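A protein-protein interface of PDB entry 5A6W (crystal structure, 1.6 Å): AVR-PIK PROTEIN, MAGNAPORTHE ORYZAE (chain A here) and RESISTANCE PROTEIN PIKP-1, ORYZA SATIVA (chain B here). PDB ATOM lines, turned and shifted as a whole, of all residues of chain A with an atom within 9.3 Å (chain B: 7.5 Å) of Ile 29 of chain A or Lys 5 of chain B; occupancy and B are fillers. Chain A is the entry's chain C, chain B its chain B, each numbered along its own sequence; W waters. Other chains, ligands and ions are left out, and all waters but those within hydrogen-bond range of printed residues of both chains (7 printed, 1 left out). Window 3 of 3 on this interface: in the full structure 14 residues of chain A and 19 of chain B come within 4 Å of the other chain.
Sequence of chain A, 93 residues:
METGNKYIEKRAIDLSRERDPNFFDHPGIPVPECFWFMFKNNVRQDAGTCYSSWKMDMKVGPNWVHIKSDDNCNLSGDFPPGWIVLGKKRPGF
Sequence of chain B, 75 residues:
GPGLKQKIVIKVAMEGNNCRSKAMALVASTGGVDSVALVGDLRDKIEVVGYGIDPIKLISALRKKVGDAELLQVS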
ATOM      1  N   PHE A  24     -16.086 -24.480 -17.910  1.00  0.00           N
ATOM      2  CA  PHE A  24     -16.859 -23.255 -17.902  1.00  0.00           C
ATOM      3  C   PHE A  24     -16.052 -22.179 -17.186  1.00  0.00           C
ATOM      4  O   PHE A  24     -15.690 -22.360 -15.999  1.00  0.00           O
ATOM      5  CB  PHE A  24     -18.205 -23.475 -17.199  1.00  0.00           C
ATOM      6  CG  PHE A  24     -19.021 -22.239 -17.051  1.00  0.00           C
ATOM      7  CD1 PHE A  24     -19.572 -21.618 -18.163  1.00  0.00           C
ATOM      8  CD2 PHE A  24     -19.192 -21.623 -15.831  1.00  0.00           C
ATOM      9  CE1 PHE A  24     -20.312 -20.501 -18.024  1.00  0.00           C
ATOM     10  CE2 PHE A  24     -19.974 -20.495 -15.686  1.00  0.00           C
ATOM     11  CZ  PHE A  24     -20.512 -19.912 -16.788  1.00  0.00           C
ATOM     12  N   ASP A  25     -15.764 -21.073 -17.881  1.00  0.00           N
ATOM     13  CA  ASP A  25     -15.054 -19.975 -17.251  1.00  0.00           C
ATOM     14  C   ASP A  25     -16.012 -19.091 -16.479  1.00  0.00           C
ATOM     15  O   ASP A  25     -16.552 -18.135 -17.012  1.00  0.00           O
ATOM     16  CB  ASP A  25     -14.212 -19.180 -18.272  1.00  0.00           C
ATOM     17  CG  ASP A  25     -13.030 -19.977 -18.809  1.00  0.00           C
ATOM     18  OD1 ASP A  25     -12.411 -20.736 -18.042  1.00  0.00           O
ATOM     19  OD2 ASP A  25     -12.677 -19.771 -19.995  1.00  0.00           O
ATOM     20  N   HIS A  26     -16.175 -19.395 -15.192  1.00  0.00           N
ATOM     21  CA  HIS A  26     -17.104 -18.657 -14.330  1.00  0.00           C
ATOM     22  C   HIS A  26     -16.809 -17.171 -14.401  1.00  0.00           C
ATOM     23  O   HIS A  26     -15.660 -16.757 -14.160  1.00  0.00           O
ATOM     24  CB  HIS A  26     -16.971 -19.179 -12.887  1.00  0.00           C
ATOM     25  CG  HIS A  26     -17.268 -20.649 -12.745  1.00  0.00           C
ATOM     26  ND1 HIS A  26     -18.504 -21.123 -12.356  1.00  0.00           N
ATOM     27  CD2 HIS A  26     -16.520 -21.738 -13.008  1.00  0.00           C
ATOM     28  CE1 HIS A  26     -18.490 -22.437 -12.366  1.00  0.00           C
ATOM     29  NE2 HIS A  26     -17.300 -22.839 -12.770  1.00  0.00           N
ATOM     30  N   PRO A  27     -17.839 -16.355 -14.665  1.00  0.00           N
ATOM     31  CA  PRO A  27     -17.503 -14.958 -14.904  1.00  0.00           C
ATOM     32  C   PRO A  27     -17.120 -14.162 -13.683  1.00  0.00           C
ATOM     33  O   PRO A  27     -16.527 -13.069 -13.836  1.00  0.00           O
ATOM     34  CB  PRO A  27     -18.780 -14.387 -15.549  1.00  0.00           C
ATOM     35  CG  PRO A  27     -19.872 -15.293 -15.168  1.00  0.00           C
ATOM     36  CD  PRO A  27     -19.239 -16.657 -15.014  1.00  0.00           C
ATOM     37  N   GLY A  28     -17.423 -14.639 -12.481  1.00  0.00           N
ATOM     38  CA  GLY A  28     -17.146 -13.831 -11.282  1.00  0.00           C
ATOM     39  C   GLY A  28     -15.779 -14.020 -10.653  1.00  0.00           C
ATOM     40  O   GLY A  28     -15.487 -13.454  -9.574  1.00  0.00           O
ATOM     41  N   ILE A  29     -14.941 -14.809 -11.318  1.00  0.00           N
ATOM     42  CA  ILE A  29     -13.584 -15.111 -10.824  1.00  0.00           C
ATOM     43  C   ILE A  29     -12.620 -15.000 -12.013  1.00  0.00           C
ATOM     44  O   ILE A  29     -13.030 -15.040 -13.154  1.00  0.00           O
ATOM     45  CB  ILE A  29     -13.489 -16.477 -10.134  1.00  0.00           C
ATOM     46  CG1 ILE A  29     -14.036 -17.617 -11.019  1.00  0.00           C
ATOM     47  CG2 ILE A  29     -14.215 -16.495  -8.803  1.00  0.00           C
ATOM     48  CD1 ILE A  29     -13.799 -18.989 -10.460  1.00  0.00           C
ATOM     49  N   PRO A  30     -11.324 -14.783 -11.741  1.00  0.00           N
ATOM     50  CA  PRO A  30     -10.390 -14.693 -12.876  1.00  0.00           C
ATOM     51  C   PRO A  30     -10.381 -15.993 -13.698  1.00  0.00           C
ATOM     52  O   PRO A  30     -10.697 -17.070 -13.188  1.00  0.00           O
ATOM     53  CB  PRO A  30      -9.019 -14.501 -12.226  1.00  0.00           C
ATOM     54  CG  PRO A  30      -9.273 -14.336 -10.776  1.00  0.00           C
ATOM     55  CD  PRO A  30     -10.709 -14.492 -10.440  1.00  0.00           C
ATOM     56  N   VAL A  31      -9.983 -15.843 -14.943  1.00  0.00           N
ATOM     57  CA  VAL A  31      -9.963 -17.023 -15.848  1.00  0.00           C
ATOM     58  C   VAL A  31      -8.746 -17.857 -15.504  1.00  0.00           C
ATOM     59  O   VAL A  31      -7.609 -17.357 -15.540  1.00  0.00           O
ATOM     60  CB  VAL A  31      -9.949 -16.569 -17.314  1.00  0.00           C
ATOM     61  CG1 VAL A  31      -9.820 -17.771 -18.240  1.00  0.00           C
ATOM     62  CG2 VAL A  31     -11.215 -15.742 -17.595  1.00  0.00           C
ATOM     63  N   PRO A  32      -8.937 -19.162 -15.240  1.00  0.00           N
ATOM     64  CA  PRO A  32      -7.784 -20.013 -14.888  1.00  0.00           C
ATOM     65  C   PRO A  32      -6.895 -20.253 -16.105  1.00  0.00           C
ATOM     66  O   PRO A  32      -7.392 -20.354 -17.243  1.00  0.00           O
ATOM     67  CB  PRO A  32      -8.417 -21.292 -14.373  1.00  0.00           C
ATOM     68  CG  PRO A  32      -9.789 -21.294 -14.979  1.00  0.00           C
ATOM     69  CD  PRO A  32     -10.225 -19.858 -15.081  1.00  0.00           C
ATOM     70  N   THR A  49     -10.040 -27.199 -15.718  1.00  0.00           N
ATOM     71  CA  THR A  49      -9.192 -26.030 -15.632  1.00  0.00           C
ATOM     72  C   THR A  49      -8.693 -25.819 -14.227  1.00  0.00           C
ATOM     73  O   THR A  49      -9.305 -26.229 -13.243  1.00  0.00           O
ATOM     74  CB  THR A  49      -9.956 -24.755 -16.045  1.00  0.00           C
ATOM     75  OG1 THR A  49     -11.132 -24.617 -15.231  1.00  0.00           O
ATOM     76  CG2 THR A  49     -10.307 -24.803 -17.515  1.00  0.00           C
ATOM     77  N   CYS A  50      -7.554 -25.127 -14.116  1.00  0.00           N
ATOM     78  CA  CYS A  50      -7.019 -24.742 -12.827  1.00  0.00           C
ATOM     79  C   CYS A  50      -6.087 -23.531 -12.960  1.00  0.00           C
ATOM     80  O   CYS A  50      -5.620 -23.214 -14.052  1.00  0.00           O
ATOM     81  CB  CYS A  50      -6.331 -25.886 -12.121  1.00  0.00           C
ATOM     82  SG  CYS A  50      -4.814 -26.529 -12.889  1.00  0.00           S
ATOM     83  N   TYR A  51      -5.847 -22.864 -11.843  1.00  0.00           N
ATOM     84  CA  TYR A  51      -4.984 -21.698 -11.877  1.00  0.00           C
ATOM     85  C   TYR A  51      -3.535 -22.086 -11.853  1.00  0.00           C
ATOM     86  O   TYR A  51      -3.129 -23.070 -11.174  1.00  0.00           O
ATOM     87  CB  TYR A  51      -5.272 -20.778 -10.685  1.00  0.00           C
ATOM     88  CG  TYR A  51      -6.620 -20.130 -10.765  1.00  0.00           C
ATOM     89  CD1 TYR A  51      -6.838 -18.985 -11.517  1.00  0.00           C
ATOM     90  CD2 TYR A  51      -7.689 -20.673 -10.075  1.00  0.00           C
ATOM     91  CE1 TYR A  51      -8.097 -18.417 -11.610  1.00  0.00           C
ATOM     92  CE2 TYR A  51      -8.963 -20.099 -10.148  1.00  0.00           C
ATOM     93  CZ  TYR A  51      -9.149 -18.982 -10.928  1.00  0.00           C
ATOM     94  OH  TYR A  51     -10.387 -18.338 -11.001  1.00  0.00           O
ATOM     95  N   TRP A  54      -0.794 -21.695  -7.883  1.00  0.00           N
ATOM     96  CA  TRP A  54      -1.941 -21.816  -6.985  1.00  0.00           C
ATOM     97  C   TRP A  54      -1.950 -23.252  -6.439  1.00  0.00           C
ATOM     98  O   TRP A  54      -0.931 -23.959  -6.513  1.00  0.00           O
ATOM     99  CB  TRP A  54      -3.252 -21.452  -7.706  1.00  0.00           C
ATOM    100  CG  TRP A  54      -4.430 -21.224  -6.785  1.00  0.00           C
ATOM    101  CD1 TRP A  54      -5.611 -21.886  -6.790  1.00  0.00           C
ATOM    102  CD2 TRP A  54      -4.510 -20.257  -5.749  1.00  0.00           C
ATOM    103  NE1 TRP A  54      -6.417 -21.416  -5.784  1.00  0.00           N
ATOM    104  CE2 TRP A  54      -5.745 -20.430  -5.111  1.00  0.00           C
ATOM    105  CE3 TRP A  54      -3.635 -19.289  -5.268  1.00  0.00           C
ATOM    106  CZ2 TRP A  54      -6.153 -19.620  -4.058  1.00  0.00           C
ATOM    107  CZ3 TRP A  54      -4.056 -18.466  -4.171  1.00  0.00           C
ATOM    108  CH2 TRP A  54      -5.274 -18.666  -3.590  1.00  0.00           C
ATOM    109  N   ARG A  90      -3.205 -23.105 -21.130  1.00  0.00           N
ATOM    110  CA  ARG A  90      -4.250 -22.842 -22.117  1.00  0.00           C
ATOM    111  C   ARG A  90      -3.706 -21.934 -23.219  1.00  0.00           C
ATOM    112  O   ARG A  90      -2.769 -21.193 -22.990  1.00  0.00           O
ATOM    113  CB  ARG A  90      -5.438 -22.181 -21.433  1.00  0.00           C
ATOM    114  CG  ARG A  90      -6.143 -23.128 -20.494  1.00  0.00           C
ATOM    115  CD  ARG A  90      -7.247 -22.468 -19.691  1.00  0.00           C
ATOM    116  NE  ARG A  90      -8.365 -22.091 -20.537  1.00  0.00           N
ATOM    117  CZ  ARG A  90      -9.501 -21.589 -20.088  1.00  0.00           C
ATOM    118  NH1 ARG A  90      -9.667 -21.315 -18.794  1.00  0.00           N
ATOM    119  NH2 ARG A  90     -10.472 -21.347 -20.935  1.00  0.00           N
ATOM    120  N   GLY B   1     -10.506 -20.171  -5.112  1.00  0.00           N
ATOM    121  CA  GLY B   1      -9.514 -19.848  -6.230  1.00  0.00           C
ATOM    122  C   GLY B   1      -8.985 -18.572  -5.659  1.00  0.00           C
ATOM    123  O   GLY B   1      -9.456 -18.133  -4.593  1.00  0.00           O
ATOM    124  N   PRO B   2      -8.011 -17.941  -6.319  1.00  0.00           N
ATOM    125  CA  PRO B   2      -7.546 -16.683  -5.731  1.00  0.00           C
ATOM    126  C   PRO B   2      -8.671 -15.683  -5.610  1.00  0.00           C
ATOM    127  O   PRO B   2      -9.546 -15.618  -6.499  1.00  0.00           O
ATOM    128  CB  PRO B   2      -6.517 -16.168  -6.729  1.00  0.00           C
ATOM    129  CG  PRO B   2      -6.376 -17.186  -7.777  1.00  0.00           C
ATOM    130  CD  PRO B   2      -7.306 -18.296  -7.567  1.00  0.00           C
ATOM    131  N   GLY B   3      -8.621 -14.865  -4.552  1.00  0.00           N
ATOM    132  CA  GLY B   3      -9.708 -13.953  -4.216  1.00  0.00           C
ATOM    133  C   GLY B   3     -10.563 -14.503  -3.104  1.00  0.00           C
ATOM    134  O   GLY B   3     -10.172 -15.397  -2.411  1.00  0.00           O
ATOM    135  N   LEU B   4     -11.776 -13.971  -2.990  1.00  0.00           N
ATOM    136  CA  LEU B   4     -12.645 -14.301  -1.904  1.00  0.00           C
ATOM    137  C   LEU B   4     -13.538 -15.491  -2.156  1.00  0.00           C
ATOM    138  O   LEU B   4     -14.030 -16.113  -1.207  1.00  0.00           O
ATOM    139  CB  LEU B   4     -13.458 -13.071  -1.526  1.00  0.00           C
ATOM    140  CG  LEU B   4     -13.731 -12.866  -0.033  1.00  0.00           C
ATOM    141  CD1 LEU B   4     -12.586 -13.228   0.913  1.00  0.00           C
ATOM    142  CD2 LEU B   4     -14.119 -11.425   0.175  1.00  0.00           C
ATOM    143  N   LYS B   5     -13.646 -15.906  -3.410  1.00  0.00           N
ATOM    144  CA  LYS B   5     -14.586 -16.922  -3.747  1.00  0.00           C
ATOM    145  C   LYS B   5     -13.975 -18.311  -3.675  1.00  0.00           C
ATOM    146  O   LYS B   5     -12.755 -18.513  -3.753  1.00  0.00           O
ATOM    147  CB  LYS B   5     -15.153 -16.720  -5.170  1.00  0.00           C
ATOM    148  CG  LYS B   5     -15.739 -15.334  -5.438  1.00  0.00           C
ATOM    149  CD  LYS B   5     -16.835 -14.986  -4.451  1.00  0.00           C
ATOM    150  CE  LYS B   5     -17.216 -13.530  -4.500  1.00  0.00           C
ATOM    151  NZ  LYS B   5     -18.219 -13.340  -5.565  1.00  0.00           N
ATOM    152  N   GLN B   6     -14.865 -19.241  -3.427  1.00  0.00           N
ATOM    153  CA  GLN B   6     -14.588 -20.661  -3.348  1.00  0.00           C
ATOM    154  C   GLN B   6     -15.021 -21.316  -4.622  1.00  0.00           C
ATOM    155  O   GLN B   6     -16.059 -20.921  -5.134  1.00  0.00           O
ATOM    156  CB  GLN B   6     -15.555 -21.240  -2.294  1.00  0.00           C
ATOM    157  CG  GLN B   6     -15.470 -20.718  -0.876  1.00  0.00           C
ATOM    158  CD  GLN B   6     -16.685 -21.165  -0.104  1.00  0.00           C
ATOM    159  OE1 GLN B   6     -17.766 -20.541  -0.198  1.00  0.00           O
ATOM    160  NE2 GLN B   6     -16.556 -22.325   0.579  1.00  0.00           N
ATOM    161  N   LYS B   7     -14.286 -22.326  -5.100  1.00  0.00           N
ATOM    162  CA  LYS B   7     -14.755 -23.248  -6.154  1.00  0.00           C
ATOM    163  C   LYS B   7     -14.798 -24.661  -5.643  1.00  0.00           C
ATOM    164  O   LYS B   7     -13.825 -25.143  -5.074  1.00  0.00           O
ATOM    165  CB  LYS B   7     -13.894 -23.168  -7.416  1.00  0.00           C
ATOM    166  CG  LYS B   7     -14.367 -24.121  -8.526  1.00  0.00           C
ATOM    167  CD  LYS B   7     -13.444 -24.154  -9.740  1.00  0.00           C
ATOM    168  CE  LYS B   7     -13.588 -22.916 -10.550  1.00  0.00           C
ATOM    169  NZ  LYS B   7     -12.674 -22.882 -11.735  1.00  0.00           N
ATOM    170  N   GLY B  32     -25.239 -17.810  -1.331  1.00  0.00           N
ATOM    171  CA  GLY B  32     -23.836 -17.465  -1.608  1.00  0.00           C
ATOM    172  C   GLY B  32     -23.344 -17.888  -2.974  1.00  0.00           C
ATOM    173  O   GLY B  32     -22.218 -17.527  -3.361  1.00  0.00           O
ATOM    174  N   VAL B  33     -24.197 -18.588  -3.732  1.00  0.00           N
ATOM    175  CA  VAL B  33     -23.809 -19.085  -5.073  1.00  0.00           C
ATOM    176  C   VAL B  33     -23.784 -17.987  -6.127  1.00  0.00           C
ATOM    177  O   VAL B  33     -24.764 -17.240  -6.317  1.00  0.00           O
ATOM    178  CB  VAL B  33     -24.670 -20.326  -5.476  1.00  0.00           C
ATOM    179  CG1 VAL B  33     -24.463 -20.727  -6.935  1.00  0.00           C
ATOM    180  CG2 VAL B  33     -24.380 -21.486  -4.566  1.00  0.00           C
ATOM    181  N   ASP B  34     -22.668 -17.835  -6.812  1.00  0.00           N
ATOM    182  CA  ASP B  34     -22.535 -16.931  -7.965  1.00  0.00           C
ATOM    183  C   ASP B  34     -22.785 -17.633  -9.299  1.00  0.00           C
ATOM    184  O   ASP B  34     -23.351 -17.033 -10.225  1.00  0.00           O
ATOM    185  CB  ASP B  34     -21.138 -16.337  -8.045  1.00  0.00           C
ATOM    186  CG  ASP B  34     -20.802 -15.495  -6.831  1.00  0.00           C
ATOM    187  OD1 ASP B  34     -21.705 -14.797  -6.334  1.00  0.00           O
ATOM    188  OD2 ASP B  34     -19.627 -15.523  -6.438  1.00  0.00           O
ATOM    189  N   SER B  35     -22.324 -18.874  -9.435  1.00  0.00           N
ATOM    190  CA  SER B  35     -22.438 -19.583 -10.742  1.00  0.00           C
ATOM    191  C   SER B  35     -22.336 -21.082 -10.534  1.00  0.00           C
ATOM    192  O   SER B  35     -21.718 -21.525  -9.575  1.00  0.00           O
ATOM    193  CB  SER B  35     -21.377 -19.105 -11.749  1.00  0.00           C
ATOM    194  OG  SER B  35     -20.063 -19.172 -11.237  1.00  0.00           O
ATOM    195  N   GLU B  47     -19.745 -27.833 -11.011  1.00  0.00           N
ATOM    196  CA  GLU B  47     -18.809 -26.918 -10.448  1.00  0.00           C
ATOM    197  C   GLU B  47     -19.577 -25.688  -9.931  1.00  0.00           C
ATOM    198  O   GLU B  47     -20.371 -25.103 -10.675  1.00  0.00           O
ATOM    199  CB  GLU B  47     -17.806 -26.608 -11.538  1.00  0.00           C
ATOM    200  CG  GLU B  47     -16.603 -25.827 -11.118  1.00  0.00           C
ATOM    201  CD  GLU B  47     -15.639 -25.738 -12.282  1.00  0.00           C
ATOM    202  OE1 GLU B  47     -15.855 -24.905 -13.180  1.00  0.00           O
ATOM    203  OE2 GLU B  47     -14.724 -26.568 -12.363  1.00  0.00           O
ATOM    204  N   VAL B  48     -19.342 -25.315  -8.668  1.00  0.00           N
ATOM    205  CA  VAL B  48     -20.084 -24.243  -7.995  1.00  0.00           C
ATOM    206  C   VAL B  48     -19.070 -23.205  -7.518  1.00  0.00           C
ATOM    207  O   VAL B  48     -18.047 -23.564  -6.874  1.00  0.00           O
ATOM    208  CB  VAL B  48     -20.839 -24.764  -6.762  1.00  0.00           C
ATOM    209  CG1 VAL B  48     -21.766 -23.670  -6.239  1.00  0.00           C
ATOM    210  CG2 VAL B  48     -21.537 -26.077  -7.071  1.00  0.00           C
ATOM    211  N   VAL B  49     -19.338 -21.918  -7.799  1.00  0.00           N
ATOM    212  CA  VAL B  49     -18.492 -20.821  -7.342  1.00  0.00           C
ATOM    213  C   VAL B  49     -19.347 -19.874  -6.535  1.00  0.00           C
ATOM    214  O   VAL B  49     -20.444 -19.560  -6.914  1.00  0.00           O
ATOM    215  CB  VAL B  49     -17.834 -20.091  -8.531  1.00  0.00           C
ATOM    216  CG1 VAL B  49     -17.143 -18.786  -8.100  1.00  0.00           C
ATOM    217  CG2 VAL B  49     -16.869 -21.048  -9.206  1.00  0.00           C
ATOM    218  N   GLY B  50     -18.807 -19.418  -5.419  1.00  0.00           N
ATOM    219  CA  GLY B  50     -19.500 -18.458  -4.590  1.00  0.00           C
ATOM    220  C   GLY B  50     -18.762 -18.164  -3.306  1.00  0.00           C
ATOM    221  O   GLY B  50     -17.581 -18.367  -3.202  1.00  0.00           O
ATOM    222  N   TYR B  51     -19.512 -17.683  -2.338  1.00  0.00           N
ATOM    223  CA  TYR B  51     -18.986 -17.238  -1.062  1.00  0.00           C
ATOM    224  C   TYR B  51     -19.873 -17.743   0.068  1.00  0.00           C
ATOM    225  O   TYR B  51     -21.083 -17.661  -0.010  1.00  0.00           O
ATOM    226  CB  TYR B  51     -18.975 -15.716  -1.032  1.00  0.00           C
ATOM    227  CG  TYR B  51     -18.391 -15.183   0.223  1.00  0.00           C
ATOM    228  CD1 TYR B  51     -17.016 -15.252   0.457  1.00  0.00           C
ATOM    229  CD2 TYR B  51     -19.209 -14.678   1.236  1.00  0.00           C
ATOM    230  CE1 TYR B  51     -16.470 -14.797   1.629  1.00  0.00           C
ATOM    231  CE2 TYR B  51     -18.660 -14.217   2.427  1.00  0.00           C
ATOM    232  CZ  TYR B  51     -17.282 -14.259   2.600  1.00  0.00           C
ATOM    233  OH  TYR B  51     -16.701 -13.815   3.785  1.00  0.00           O
ATOM    234  N   GLY B  52     -19.267 -18.232   1.144  1.00  0.00           N
ATOM    235  CA  GLY B  52     -20.034 -18.707   2.280  1.00  0.00           C
ATOM    236  C   GLY B  52     -20.786 -20.001   2.044  1.00  0.00           C
ATOM    237  O   GLY B  52     -21.838 -20.233   2.682  1.00  0.00           O
ATOM    238  N   SER B  75     -10.998 -25.560  -4.276  1.00  0.00           N
ATOM    239  CA  SER B  75      -9.892 -24.698  -4.647  1.00  0.00           C
ATOM    240  C   SER B  75     -10.270 -23.234  -4.554  1.00  0.00           C
ATOM    241  O   SER B  75     -11.432 -22.933  -4.314  1.00  0.00           O
ATOM    242  CB  SER B  75      -9.409 -25.024  -6.043  1.00  0.00           C
ATOM    243  OG  SER B  75     -10.420 -24.810  -6.963  1.00  0.00           O
ATOM    244  OXT SER B  75      -9.365 -22.377  -4.602  1.00  0.00           O
HETATM  245  O   HOH W   1     -18.963 -16.663 -11.155  1.00  0.00           O
HETATM  246  O   HOH W   2     -12.306 -25.464 -12.928  1.00  0.00           O
HETATM  247  O   HOH W   3     -14.474 -25.076 -15.629  1.00  0.00           O
HETATM  248  O   HOH W   4     -18.080 -15.378  -8.667  1.00  0.00           O
HETATM  249  O   HOH W   5     -10.861 -17.626  -8.184  1.00  0.00           O
HETATM  250  O   HOH W   6     -13.457 -20.719 -13.922  1.00  0.00           O
HETATM  251  O   HOH W   7      -7.010 -23.146  -3.187  1.00  0.00           O
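Phe 24 of chain A touches Glu 47 of chain B (O to OE1, 3.8 Å). CG2 of Val 49 of chain B touches ND1 of His 26 of chain A, 3.5 Å away. Ile 29 of chain A touches Lys 5 of chain B (CG2 to CB, 3.8 Å). Ile 29 of chain A touches Lys 7 of chain B. Ile 29 of chain A touches Val 49 of chain B (CG2 to CG1, 3.8 Å). Tyr 51 of chain A touches Gly 1 of chain B (CE2 to CA, 3.96 Å). Tyr 51 of chain A touches Pro 2 of chain B. Trp 54 of chain A touches Gly 1 of chain B. Trp 54 of chain A touches Pro 2 of chain B (CZ2 to N, 3.4 Å).
ND1 of His 26 of chain A sits at hydrogen-bond distance from OG of Ser 35 of chain B, 2.7 Å away. The side-chain carboxylate (OE1) of Glu 47 of chain B sits at hydrogen-bond distance from a ring nitrogen (NE2) of His 26 of chain A, at 2.6 Å. NE1 of Trp 54 of chain A lies within hydrogen-bond range of OXT of Ser 75 of chain B, 3.3 Å away.
Of the printed residues of chain B, Ile 29 of chain A touches Lys 5 (3.8 Å), Lys 7 (3.9 Å) and Val 49 (3.8 Å). Of chain A, only Ile 29 comes within 4 Å of Lys 5 of chain B. No residue of chain B comes within 4 Å of Gly 28 of chain A. Gly 1 of chain B touches two residues of chain A. No residue of chain A comes within 4 Å of Gly 50 of chain B. Of the printed residues of chain A, Val 49 of chain B touches His 26 (3.5 Å) and Ile 29 (3.8 Å). Printed residues of chain A within 4 Å of Ser 35 of chain B: His 26 (2.7 Å). Gln 6 of chain B touches none of the printed residues of chain A. Gly 32 of chain B touches none of the printed residues of chain A. The nearest residue of chain B that does not touch Ile 29 of chain A is Pro 2 of chain B (5.3 Å).
Water W2 lies within hydrogen-bond range of the side-chain carboxylate of Glu 47 of chain B (2.7 Å), the side-chain hydroxyl of Thr 49 of chain A (2.7 Å) and the side-chain amino group of Lys 7 of chain B (2.9 Å). Water W4 lies within hydrogen-bond range of OD2 of Asp 34 of chain B (2.7 Å) and O of Gly 28 of chain A (3.4 Å). Water W1 lies within hydrogen-bond range of the side-chain hydroxyl (OG) of Ser 35 of chain B (2.7 Å) and the backbone NH (N) of Gly 28 of chain A (2.9 Å). Water W3 lies within hydrogen-bond range of OE1 of Glu 47 of chain B (2.8 Å), N of Phe 24 of chain A (2.9 Å) and OG1 of Thr 49 of chain A (3.4 Å). Water W7 bridges the chain-end carboxylate (OXT) of Ser 75 of chain B (2.9 Å) and the indole nitrogen (NE1) of Trp 54 of chain A (3.2 Å). Water W5 bridges O of Pro 2 of chain B (2.9 Å) and OH of Tyr 51 of chain A (2.9 Å).
The backbone NH of Gly 1 of chain B lies within hydrogen-bond range of the chain-end carboxylate of Ser 75 of chain B (2.5 Å). OD2 of Asp 34 of chain B is in salt-bridge range of NZ of Lys 5 of chain B (2.7 Å). O of Lys 7 of chain B is in hydrogen-bond range of N of Ser 75 of chain B, 3.0 Å away. The backbone NH (N) of Asp 34 of chain B lies within hydrogen-bond range of the backbone carbonyl oxygen (O) of Val 49 of chain B (2.8 Å). O of Ser 35 of chain B is in hydrogen-bond range of N of Val 49 of chain B (3.0 Å). OH of Tyr 51 of chain A lies within hydrogen-bond range of O of Pro 30 of chain A (2.5 Å).
Of the 14 printed residues of chain A, 5 touch a printed residue of chain B. Printed residues of chain A that touch a printed residue of chain B: Phe 24, His 26, Ile 29, Tyr 51 and Trp 54. Hydrophobic or aromatic side chains of chain A that line the printed part of chain B: His 26, Ile 29, Tyr 51 and Trp 54. Among the printed residues, no Asp or Glu carboxylate lies within 4 Å of a Lys or Arg side-chain nitrogen of the other chain.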
